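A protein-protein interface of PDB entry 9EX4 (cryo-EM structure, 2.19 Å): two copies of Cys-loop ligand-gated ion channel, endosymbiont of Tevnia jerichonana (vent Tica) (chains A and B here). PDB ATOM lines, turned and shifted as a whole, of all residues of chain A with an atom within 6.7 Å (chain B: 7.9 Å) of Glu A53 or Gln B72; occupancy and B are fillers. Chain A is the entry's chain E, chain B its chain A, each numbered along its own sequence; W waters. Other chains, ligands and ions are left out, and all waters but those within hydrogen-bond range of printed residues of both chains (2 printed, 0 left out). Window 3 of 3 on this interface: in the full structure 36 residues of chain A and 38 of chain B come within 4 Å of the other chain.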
ATOM      1  N   PHE A  47      15.134  10.374  -0.602  1.00  0.00           N
ATOM      2  CA  PHE A  47      14.489   9.714  -1.728  1.00  0.00           C
ATOM      3  C   PHE A  47      13.019   9.500  -1.404  1.00  0.00           C
ATOM      4  O   PHE A  47      12.569   9.711  -0.275  1.00  0.00           O
ATOM      5  CB  PHE A  47      15.172   8.382  -2.062  1.00  0.00           C
ATOM      6  CG  PHE A  47      15.043   7.342  -0.983  1.00  0.00           C
ATOM      7  CD1 PHE A  47      15.947   7.299   0.068  1.00  0.00           C
ATOM      8  CD2 PHE A  47      14.025   6.404  -1.019  1.00  0.00           C
ATOM      9  CE1 PHE A  47      15.833   6.345   1.062  1.00  0.00           C
ATOM     10  CE2 PHE A  47      13.905   5.449  -0.028  1.00  0.00           C
ATOM     11  CZ  PHE A  47      14.810   5.419   1.013  1.00  0.00           C
ATOM     12  N   GLU A  48      12.269   9.073  -2.419  1.00  0.00           N
ATOM     13  CA  GLU A  48      10.862   8.724  -2.279  1.00  0.00           C
ATOM     14  C   GLU A  48      10.669   7.279  -2.716  1.00  0.00           C
ATOM     15  O   GLU A  48      11.071   6.903  -3.821  1.00  0.00           O
ATOM     16  CB  GLU A  48       9.973   9.655  -3.109  1.00  0.00           C
ATOM     17  CG  GLU A  48      10.033  11.114  -2.686  1.00  0.00           C
ATOM     18  CD  GLU A  48       9.159  12.002  -3.546  1.00  0.00           C
ATOM     19  OE1 GLU A  48       8.625  11.509  -4.562  1.00  0.00           O
ATOM     20  OE2 GLU A  48       9.006  13.196  -3.209  1.00  0.00           O
ATOM     21  N   HIS A  49      10.055   6.477  -1.851  1.00  0.00           N
ATOM     22  CA  HIS A  49       9.889   5.058  -2.127  1.00  0.00           C
ATOM     23  C   HIS A  49       8.792   4.829  -3.159  1.00  0.00           C
ATOM     24  O   HIS A  49       7.755   5.498  -3.148  1.00  0.00           O
ATOM     25  CB  HIS A  49       9.562   4.296  -0.841  1.00  0.00           C
ATOM     26  CG  HIS A  49       8.201   4.590  -0.292  1.00  0.00           C
ATOM     27  ND1 HIS A  49       7.929   5.706   0.471  1.00  0.00           N
ATOM     28  CD2 HIS A  49       7.033   3.913  -0.395  1.00  0.00           C
ATOM     29  CE1 HIS A  49       6.654   5.703   0.813  1.00  0.00           C
ATOM     30  NE2 HIS A  49       6.087   4.625   0.301  1.00  0.00           N
ATOM     31  N   ALA A  50       9.034   3.879  -4.059  1.00  0.00           N
ATOM     32  CA  ALA A  50       8.038   3.472  -5.032  1.00  0.00           C
ATOM     33  C   ALA A  50       7.035   2.514  -4.388  1.00  0.00           C
ATOM     34  O   ALA A  50       7.351   1.856  -3.393  1.00  0.00           O
ATOM     35  CB  ALA A  50       8.706   2.800  -6.228  1.00  0.00           C
ATOM     36  N   PRO A  51       5.816   2.431  -4.923  1.00  0.00           N
ATOM     37  CA  PRO A  51       4.837   1.489  -4.368  1.00  0.00           C
ATOM     38  C   PRO A  51       5.342   0.056  -4.445  1.00  0.00           C
ATOM     39  O   PRO A  51       5.950  -0.359  -5.435  1.00  0.00           O
ATOM     40  CB  PRO A  51       3.596   1.701  -5.245  1.00  0.00           C
ATOM     41  CG  PRO A  51       4.106   2.361  -6.488  1.00  0.00           C
ATOM     42  CD  PRO A  51       5.251   3.211  -6.038  1.00  0.00           C
ATOM     43  N   GLY A  52       5.082  -0.704  -3.381  1.00  0.00           N
ATOM     44  CA  GLY A  52       5.557  -2.064  -3.274  1.00  0.00           C
ATOM     45  C   GLY A  52       6.960  -2.213  -2.725  1.00  0.00           C
ATOM     46  O   GLY A  52       7.418  -3.348  -2.544  1.00  0.00           O
ATOM     47  N   GLU A  53       7.658  -1.105  -2.454  1.00  0.00           N
ATOM     48  CA  GLU A  53       9.019  -1.128  -1.949  1.00  0.00           C
ATOM     49  C   GLU A  53       9.057  -0.743  -0.472  1.00  0.00           C
ATOM     50  O   GLU A  53       8.203   0.014   0.000  1.00  0.00           O
ATOM     51  CB  GLU A  53       9.913  -0.171  -2.747  1.00  0.00           C
ATOM     52  CG  GLU A  53      10.057  -0.541  -4.214  1.00  0.00           C
ATOM     53  CD  GLU A  53      10.942   0.426  -4.975  1.00  0.00           C
ATOM     54  OE1 GLU A  53      11.329   1.464  -4.396  1.00  0.00           O
ATOM     55  OE2 GLU A  53      11.250   0.150  -6.153  1.00  0.00           O
ATOM     56  N   PRO A  54      10.030  -1.249   0.282  1.00  0.00           N
ATOM     57  CA  PRO A  54      10.120  -0.899   1.704  1.00  0.00           C
ATOM     58  C   PRO A  54      10.502   0.559   1.904  1.00  0.00           C
ATOM     59  O   PRO A  54      11.092   1.208   1.038  1.00  0.00           O
ATOM     60  CB  PRO A  54      11.210  -1.837   2.234  1.00  0.00           C
ATOM     61  CG  PRO A  54      12.035  -2.165   1.036  1.00  0.00           C
ATOM     62  CD  PRO A  54      11.074  -2.210  -0.115  1.00  0.00           C
ATOM     63  N   LYS A  55      10.148   1.073   3.083  1.00  0.00           N
ATOM     64  CA  LYS A  55      10.430   2.462   3.422  1.00  0.00           C
ATOM     65  C   LYS A  55      11.903   2.705   3.726  1.00  0.00           C
ATOM     66  O   LYS A  55      12.343   3.860   3.724  1.00  0.00           O
ATOM     67  CB  LYS A  55       9.563   2.890   4.611  1.00  0.00           C
ATOM     68  CG  LYS A  55       9.466   4.394   4.820  1.00  0.00           C
ATOM     69  CD  LYS A  55       8.184   4.771   5.550  1.00  0.00           C
ATOM     70  CE  LYS A  55       8.061   4.044   6.879  1.00  0.00           C
ATOM     71  NZ  LYS A  55       9.152   4.411   7.821  1.00  0.00           N
ATOM     72  N   HIS A  56      12.674   1.649   3.972  1.00  0.00           N
ATOM     73  CA  HIS A  56      14.106   1.750   4.208  1.00  0.00           C
ATOM     74  C   HIS A  56      14.854   0.882   3.205  1.00  0.00           C
ATOM     75  O   HIS A  56      14.365  -0.172   2.787  1.00  0.00           O
ATOM     76  CB  HIS A  56      14.472   1.331   5.638  1.00  0.00           C
ATOM     77  CG  HIS A  56      13.982   2.276   6.690  1.00  0.00           C
ATOM     78  ND1 HIS A  56      12.643   2.514   6.914  1.00  0.00           N
ATOM     79  CD2 HIS A  56      14.653   3.043   7.581  1.00  0.00           C
ATOM     80  CE1 HIS A  56      12.510   3.386   7.897  1.00  0.00           C
ATOM     81  NE2 HIS A  56      13.716   3.723   8.319  1.00  0.00           N
ATOM     82  N   ARG A  57      16.045   1.332   2.824  1.00  0.00           N
ATOM     83  CA  ARG A  57      16.871   0.645   1.841  1.00  0.00           C
ATOM     84  C   ARG A  57      18.107   0.060   2.511  1.00  0.00           C
ATOM     85  O   ARG A  57      18.679   0.667   3.421  1.00  0.00           O
ATOM     86  CB  ARG A  57      17.287   1.596   0.714  1.00  0.00           C
ATOM     87  CG  ARG A  57      16.127   2.090  -0.135  1.00  0.00           C
ATOM     88  CD  ARG A  57      16.603   2.998  -1.257  1.00  0.00           C
ATOM     89  NE  ARG A  57      15.509   3.403  -2.131  1.00  0.00           N
ATOM     90  CZ  ARG A  57      15.643   4.203  -3.180  1.00  0.00           C
ATOM     91  NH1 ARG A  57      16.817   4.711  -3.517  1.00  0.00           N
ATOM     92  NH2 ARG A  57      14.573   4.501  -3.910  1.00  0.00           N
ATOM     93  N   THR A  58      18.510  -1.122   2.056  1.00  0.00           N
ATOM     94  CA  THR A  58      19.657  -1.839   2.598  1.00  0.00           C
ATOM     95  C   THR A  58      20.764  -1.882   1.553  1.00  0.00           C
ATOM     96  O   THR A  58      20.506  -2.185   0.383  1.00  0.00           O
ATOM     97  CB  THR A  58      19.268  -3.259   3.017  1.00  0.00           C
ATOM     98  OG1 THR A  58      18.134  -3.207   3.892  1.00  0.00           O
ATOM     99  CG2 THR A  58      20.421  -3.940   3.740  1.00  0.00           C
ATOM    100  N   TYR A  59      21.990  -1.580   1.977  1.00  0.00           N
ATOM    101  CA  TYR A  59      23.133  -1.509   1.079  1.00  0.00           C
ATOM    102  C   TYR A  59      24.316  -2.266   1.663  1.00  0.00           C
ATOM    103  O   TYR A  59      24.442  -2.419   2.881  1.00  0.00           O
ATOM    104  CB  TYR A  59      23.565  -0.058   0.818  1.00  0.00           C
ATOM    105  CG  TYR A  59      22.603   0.756  -0.013  1.00  0.00           C
ATOM    106  CD1 TYR A  59      22.634   0.700  -1.400  1.00  0.00           C
ATOM    107  CD2 TYR A  59      21.676   1.598   0.587  1.00  0.00           C
ATOM    108  CE1 TYR A  59      21.762   1.448  -2.165  1.00  0.00           C
ATOM    109  CE2 TYR A  59      20.801   2.351  -0.169  1.00  0.00           C
ATOM    110  CZ  TYR A  59      20.848   2.273  -1.545  1.00  0.00           C
ATOM    111  OH  TYR A  59      19.977   3.020  -2.303  1.00  0.00           O
ATOM    112  N   LEU B  44       8.907 -12.416  -4.700  1.00  0.00           N
ATOM    113  CA  LEU B  44       9.378 -11.464  -5.700  1.00  0.00           C
ATOM    114  C   LEU B  44      10.524 -12.004  -6.547  1.00  0.00           C
ATOM    115  O   LEU B  44      10.885 -11.367  -7.541  1.00  0.00           O
ATOM    116  CB  LEU B  44       9.810 -10.163  -5.021  1.00  0.00           C
ATOM    117  CG  LEU B  44       8.709  -9.367  -4.316  1.00  0.00           C
ATOM    118  CD1 LEU B  44       9.279  -8.110  -3.679  1.00  0.00           C
ATOM    119  CD2 LEU B  44       7.593  -9.020  -5.289  1.00  0.00           C
ATOM    120  N   LEU B  65      23.707 -10.981  -4.132  1.00  0.00           N
ATOM    121  CA  LEU B  65      23.551  -9.728  -3.400  1.00  0.00           C
ATOM    122  C   LEU B  65      23.305  -8.560  -4.347  1.00  0.00           C
ATOM    123  O   LEU B  65      22.482  -7.681  -4.062  1.00  0.00           O
ATOM    124  CB  LEU B  65      24.780  -9.466  -2.529  1.00  0.00           C
ATOM    125  CG  LEU B  65      24.994 -10.426  -1.358  1.00  0.00           C
ATOM    126  CD1 LEU B  65      26.219 -10.027  -0.549  1.00  0.00           C
ATOM    127  CD2 LEU B  65      23.757 -10.482  -0.475  1.00  0.00           C
ATOM    128  N   LYS B  66      24.014  -8.530  -5.479  1.00  0.00           N
ATOM    129  CA  LYS B  66      23.788  -7.475  -6.462  1.00  0.00           C
ATOM    130  C   LYS B  66      22.374  -7.539  -7.027  1.00  0.00           C
ATOM    131  O   LYS B  66      21.729  -6.504  -7.224  1.00  0.00           O
ATOM    132  CB  LYS B  66      24.821  -7.569  -7.587  1.00  0.00           C
ATOM    133  CG  LYS B  66      26.232  -7.196  -7.165  1.00  0.00           C
ATOM    134  CD  LYS B  66      27.203  -7.306  -8.329  1.00  0.00           C
ATOM    135  CE  LYS B  66      28.615  -6.935  -7.906  1.00  0.00           C
ATOM    136  NZ  LYS B  66      29.575  -7.027  -9.041  1.00  0.00           N
ATOM    137  N   LEU B  67      21.876  -8.748  -7.297  1.00  0.00           N
ATOM    138  CA  LEU B  67      20.508  -8.898  -7.782  1.00  0.00           C
ATOM    139  C   LEU B  67      19.499  -8.412  -6.748  1.00  0.00           C
ATOM    140  O   LEU B  67      18.528  -7.725  -7.090  1.00  0.00           O
ATOM    141  CB  LEU B  67      20.240 -10.358  -8.148  1.00  0.00           C
ATOM    142  CG  LEU B  67      18.821 -10.707  -8.602  1.00  0.00           C
ATOM    143  CD1 LEU B  67      18.484 -10.006  -9.909  1.00  0.00           C
ATOM    144  CD2 LEU B  67      18.653 -12.212  -8.736  1.00  0.00           C
ATOM    145  N   LEU B  68      19.715  -8.757  -5.476  1.00  0.00           N
ATOM    146  CA  LEU B  68      18.813  -8.297  -4.423  1.00  0.00           C
ATOM    147  C   LEU B  68      18.830  -6.777  -4.308  1.00  0.00           C
ATOM    148  O   LEU B  68      17.780  -6.149  -4.127  1.00  0.00           O
ATOM    149  CB  LEU B  68      19.183  -8.937  -3.087  1.00  0.00           C
ATOM    150  CG  LEU B  68      18.890 -10.429  -2.922  1.00  0.00           C
ATOM    151  CD1 LEU B  68      19.155 -10.860  -1.490  1.00  0.00           C
ATOM    152  CD2 LEU B  68      17.459 -10.745  -3.326  1.00  0.00           C
ATOM    153  N   GLU B  69      20.015  -6.169  -4.402  1.00  0.00           N
ATOM    154  CA  GLU B  69      20.104  -4.713  -4.348  1.00  0.00           C
ATOM    155  C   GLU B  69      19.412  -4.068  -5.544  1.00  0.00           C
ATOM    156  O   GLU B  69      18.748  -3.036  -5.400  1.00  0.00           O
ATOM    157  CB  GLU B  69      21.567  -4.278  -4.273  1.00  0.00           C
ATOM    158  CG  GLU B  69      22.216  -4.531  -2.923  1.00  0.00           C
ATOM    159  CD  GLU B  69      23.685  -4.163  -2.908  1.00  0.00           C
ATOM    160  OE1 GLU B  69      24.327  -4.243  -3.976  1.00  0.00           O
ATOM    161  OE2 GLU B  69      24.196  -3.789  -1.832  1.00  0.00           O
ATOM    162  N   GLU B  70      19.562  -4.657  -6.733  1.00  0.00           N
ATOM    163  CA  GLU B  70      18.885  -4.127  -7.912  1.00  0.00           C
ATOM    164  C   GLU B  70      17.371  -4.212  -7.765  1.00  0.00           C
ATOM    165  O   GLU B  70      16.649  -3.285  -8.150  1.00  0.00           O
ATOM    166  CB  GLU B  70      19.344  -4.873  -9.166  1.00  0.00           C
ATOM    167  CG  GLU B  70      20.771  -4.562  -9.587  1.00  0.00           C
ATOM    168  CD  GLU B  70      21.209  -5.363 -10.796  1.00  0.00           C
ATOM    169  OE1 GLU B  70      20.454  -6.262 -11.223  1.00  0.00           O
ATOM    170  OE2 GLU B  70      22.310  -5.095 -11.322  1.00  0.00           O
ATOM    171  N   LYS B  71      16.871  -5.316  -7.208  1.00  0.00           N
ATOM    172  CA  LYS B  71      15.439  -5.447  -6.969  1.00  0.00           C
ATOM    173  C   LYS B  71      14.990  -4.778  -5.675  1.00  0.00           C
ATOM    174  O   LYS B  71      13.783  -4.726  -5.416  1.00  0.00           O
ATOM    175  CB  LYS B  71      15.039  -6.924  -6.953  1.00  0.00           C
ATOM    176  CG  LYS B  71      15.173  -7.613  -8.303  1.00  0.00           C
ATOM    177  CD  LYS B  71      14.675  -9.047  -8.247  1.00  0.00           C
ATOM    178  CE  LYS B  71      14.762  -9.711  -9.612  1.00  0.00           C
ATOM    179  NZ  LYS B  71      14.242 -11.105  -9.587  1.00  0.00           N
ATOM    180  N   GLN B  72      15.927  -4.272  -4.870  1.00  0.00           N
ATOM    181  CA  GLN B  72      15.628  -3.578  -3.615  1.00  0.00           C
ATOM    182  C   GLN B  72      14.811  -4.467  -2.674  1.00  0.00           C
ATOM    183  O   GLN B  72      13.675  -4.159  -2.307  1.00  0.00           O
ATOM    184  CB  GLN B  72      14.917  -2.246  -3.880  1.00  0.00           C
ATOM    185  CG  GLN B  72      15.741  -1.255  -4.686  1.00  0.00           C
ATOM    186  CD  GLN B  72      15.063   0.093  -4.822  1.00  0.00           C
ATOM    187  OE1 GLN B  72      14.007   0.331  -4.238  1.00  0.00           O
ATOM    188  NE2 GLN B  72      15.670   0.986  -5.597  1.00  0.00           N
ATOM    189  N   ILE B  73      15.420  -5.585  -2.284  1.00  0.00           N
ATOM    190  CA  ILE B  73      14.805  -6.555  -1.387  1.00  0.00           C
ATOM    191  C   ILE B  73      15.691  -6.702  -0.157  1.00  0.00           C
ATOM    192  O   ILE B  73      16.900  -6.932  -0.281  1.00  0.00           O
ATOM    193  CB  ILE B  73      14.596  -7.915  -2.078  1.00  0.00           C
ATOM    194  CG1 ILE B  73      13.660  -7.764  -3.279  1.00  0.00           C
ATOM    195  CG2 ILE B  73      14.048  -8.936  -1.095  1.00  0.00           C
ATOM    196  CD1 ILE B  73      13.390  -9.060  -4.012  1.00  0.00           C
ATOM    197  N   ARG B  74      15.090  -6.567   1.021  1.00  0.00           N
ATOM    198  CA  ARG B  74      15.820  -6.708   2.273  1.00  0.00           C
ATOM    199  C   ARG B  74      16.135  -8.174   2.543  1.00  0.00           C
ATOM    200  O   ARG B  74      15.278  -9.048   2.387  1.00  0.00           O
ATOM    201  CB  ARG B  74      15.007  -6.131   3.431  1.00  0.00           C
ATOM    202  CG  ARG B  74      15.765  -6.038   4.744  1.00  0.00           C
ATOM    203  CD  ARG B  74      14.810  -5.883   5.918  1.00  0.00           C
ATOM    204  NE  ARG B  74      13.782  -4.882   5.662  1.00  0.00           N
ATOM    205  CZ  ARG B  74      13.886  -3.601   5.983  1.00  0.00           C
ATOM    206  NH1 ARG B  74      14.969  -3.121   6.573  1.00  0.00           N
ATOM    207  NH2 ARG B  74      12.878  -2.779   5.705  1.00  0.00           N
ATOM    208  N   TRP B  75      17.380  -8.442   2.952  1.00  0.00           N
ATOM    209  CA  TRP B  75      17.779  -9.802   3.274  1.00  0.00           C
ATOM    210  C   TRP B  75      17.954  -9.973   4.782  1.00  0.00           C
ATOM    211  O   TRP B  75      18.312  -9.021   5.483  1.00  0.00           O
ATOM    212  CB  TRP B  75      19.083 -10.184   2.561  1.00  0.00           C
ATOM    213  CG  TRP B  75      20.247  -9.289   2.868  1.00  0.00           C
ATOM    214  CD1 TRP B  75      21.078  -9.366   3.946  1.00  0.00           C
ATOM    215  CD2 TRP B  75      20.719  -8.192   2.074  1.00  0.00           C
ATOM    216  NE1 TRP B  75      22.033  -8.381   3.879  1.00  0.00           N
ATOM    217  CE2 TRP B  75      21.835  -7.646   2.739  1.00  0.00           C
ATOM    218  CE3 TRP B  75      20.304  -7.616   0.869  1.00  0.00           C
ATOM    219  CZ2 TRP B  75      22.541  -6.554   2.241  1.00  0.00           C
ATOM    220  CZ3 TRP B  75      21.007  -6.531   0.376  1.00  0.00           C
ATOM    221  CH2 TRP B  75      22.113  -6.011   1.060  1.00  0.00           C
HETATM  222  O   HOH W   1      16.958  -1.757   5.830  1.00  0.00           O
HETATM  223  O   HOH W   2      18.215  -4.356  -0.860  1.00  0.00           O
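OE1 of Glu A53 lies close to OE1 of Gln B72 (2.9 Å).
OE1 of Glu A53 sits at hydrogen-bond distance from N of Ala A50, 3.3 Å away.
Among the printed residues, merely in contact across the chains: Thr A58 with Trp B75 (3.7 Å), Thr A58 with Arg B74 (3.8 Å), Tyr A59 with Glu B69 (3.8 Å), Pro A54 with Gln B72 (3.9 Å) and Pro A54 with Arg B74 (3.96 Å).
No residue of chain B comes within 4 Å of Gly A52.
Printed residues of chain B within 4 Å of Glu A53: Gln B72.
Of the printed residues of chain B, Thr A58 touches Arg B74 (3.8 Å) and Trp B75 (3.7 Å).
Leu B44 touches none of the printed residues of chain A.
Leu B65 touches none of the printed residues of chain A.
Of the printed residues of chain A, Gln B72 touches Glu A53 (2.9 Å) and Pro A54 (3.9 Å).
Printed residues of chain A within 4 Å of Arg B74: Pro A54 (3.96 Å) and Thr A58 (3.8 Å).
Printed residues of chain A within 4 Å of Trp B75: Thr A58 (3.7 Å).
The nearest residue of chain B that does not touch Glu A53 is Lys B71 (5.5 Å).
The nearest printed residue of chain A that does not touch Gln B72 is Arg A57 (4.02 Å).
The nearest printed residue of chain B that does not touch Thr A58 is Glu B69 (4.4 Å).
Of the 12 printed residues of chain B, 4 touch a printed residue of chain A.
Hydrophobic or aromatic side chains of chain B within 4 Å of the printed part of chain A: Trp B75.
Hydrophobic or aromatic side chains of chain A within 4 Å of the printed part of chain B: Pro A54.
No position is printed for both chains.
Water W1 lies within hydrogen-bond range of NH1 of Arg B74 and OG1 of Thr A58.
Water W2 lies within hydrogen-bond range of the backbone carbonyl oxygen of Ile B73 (2.9 Å) and the backbone carbonyl oxygen of Thr A58 (3.4 Å).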
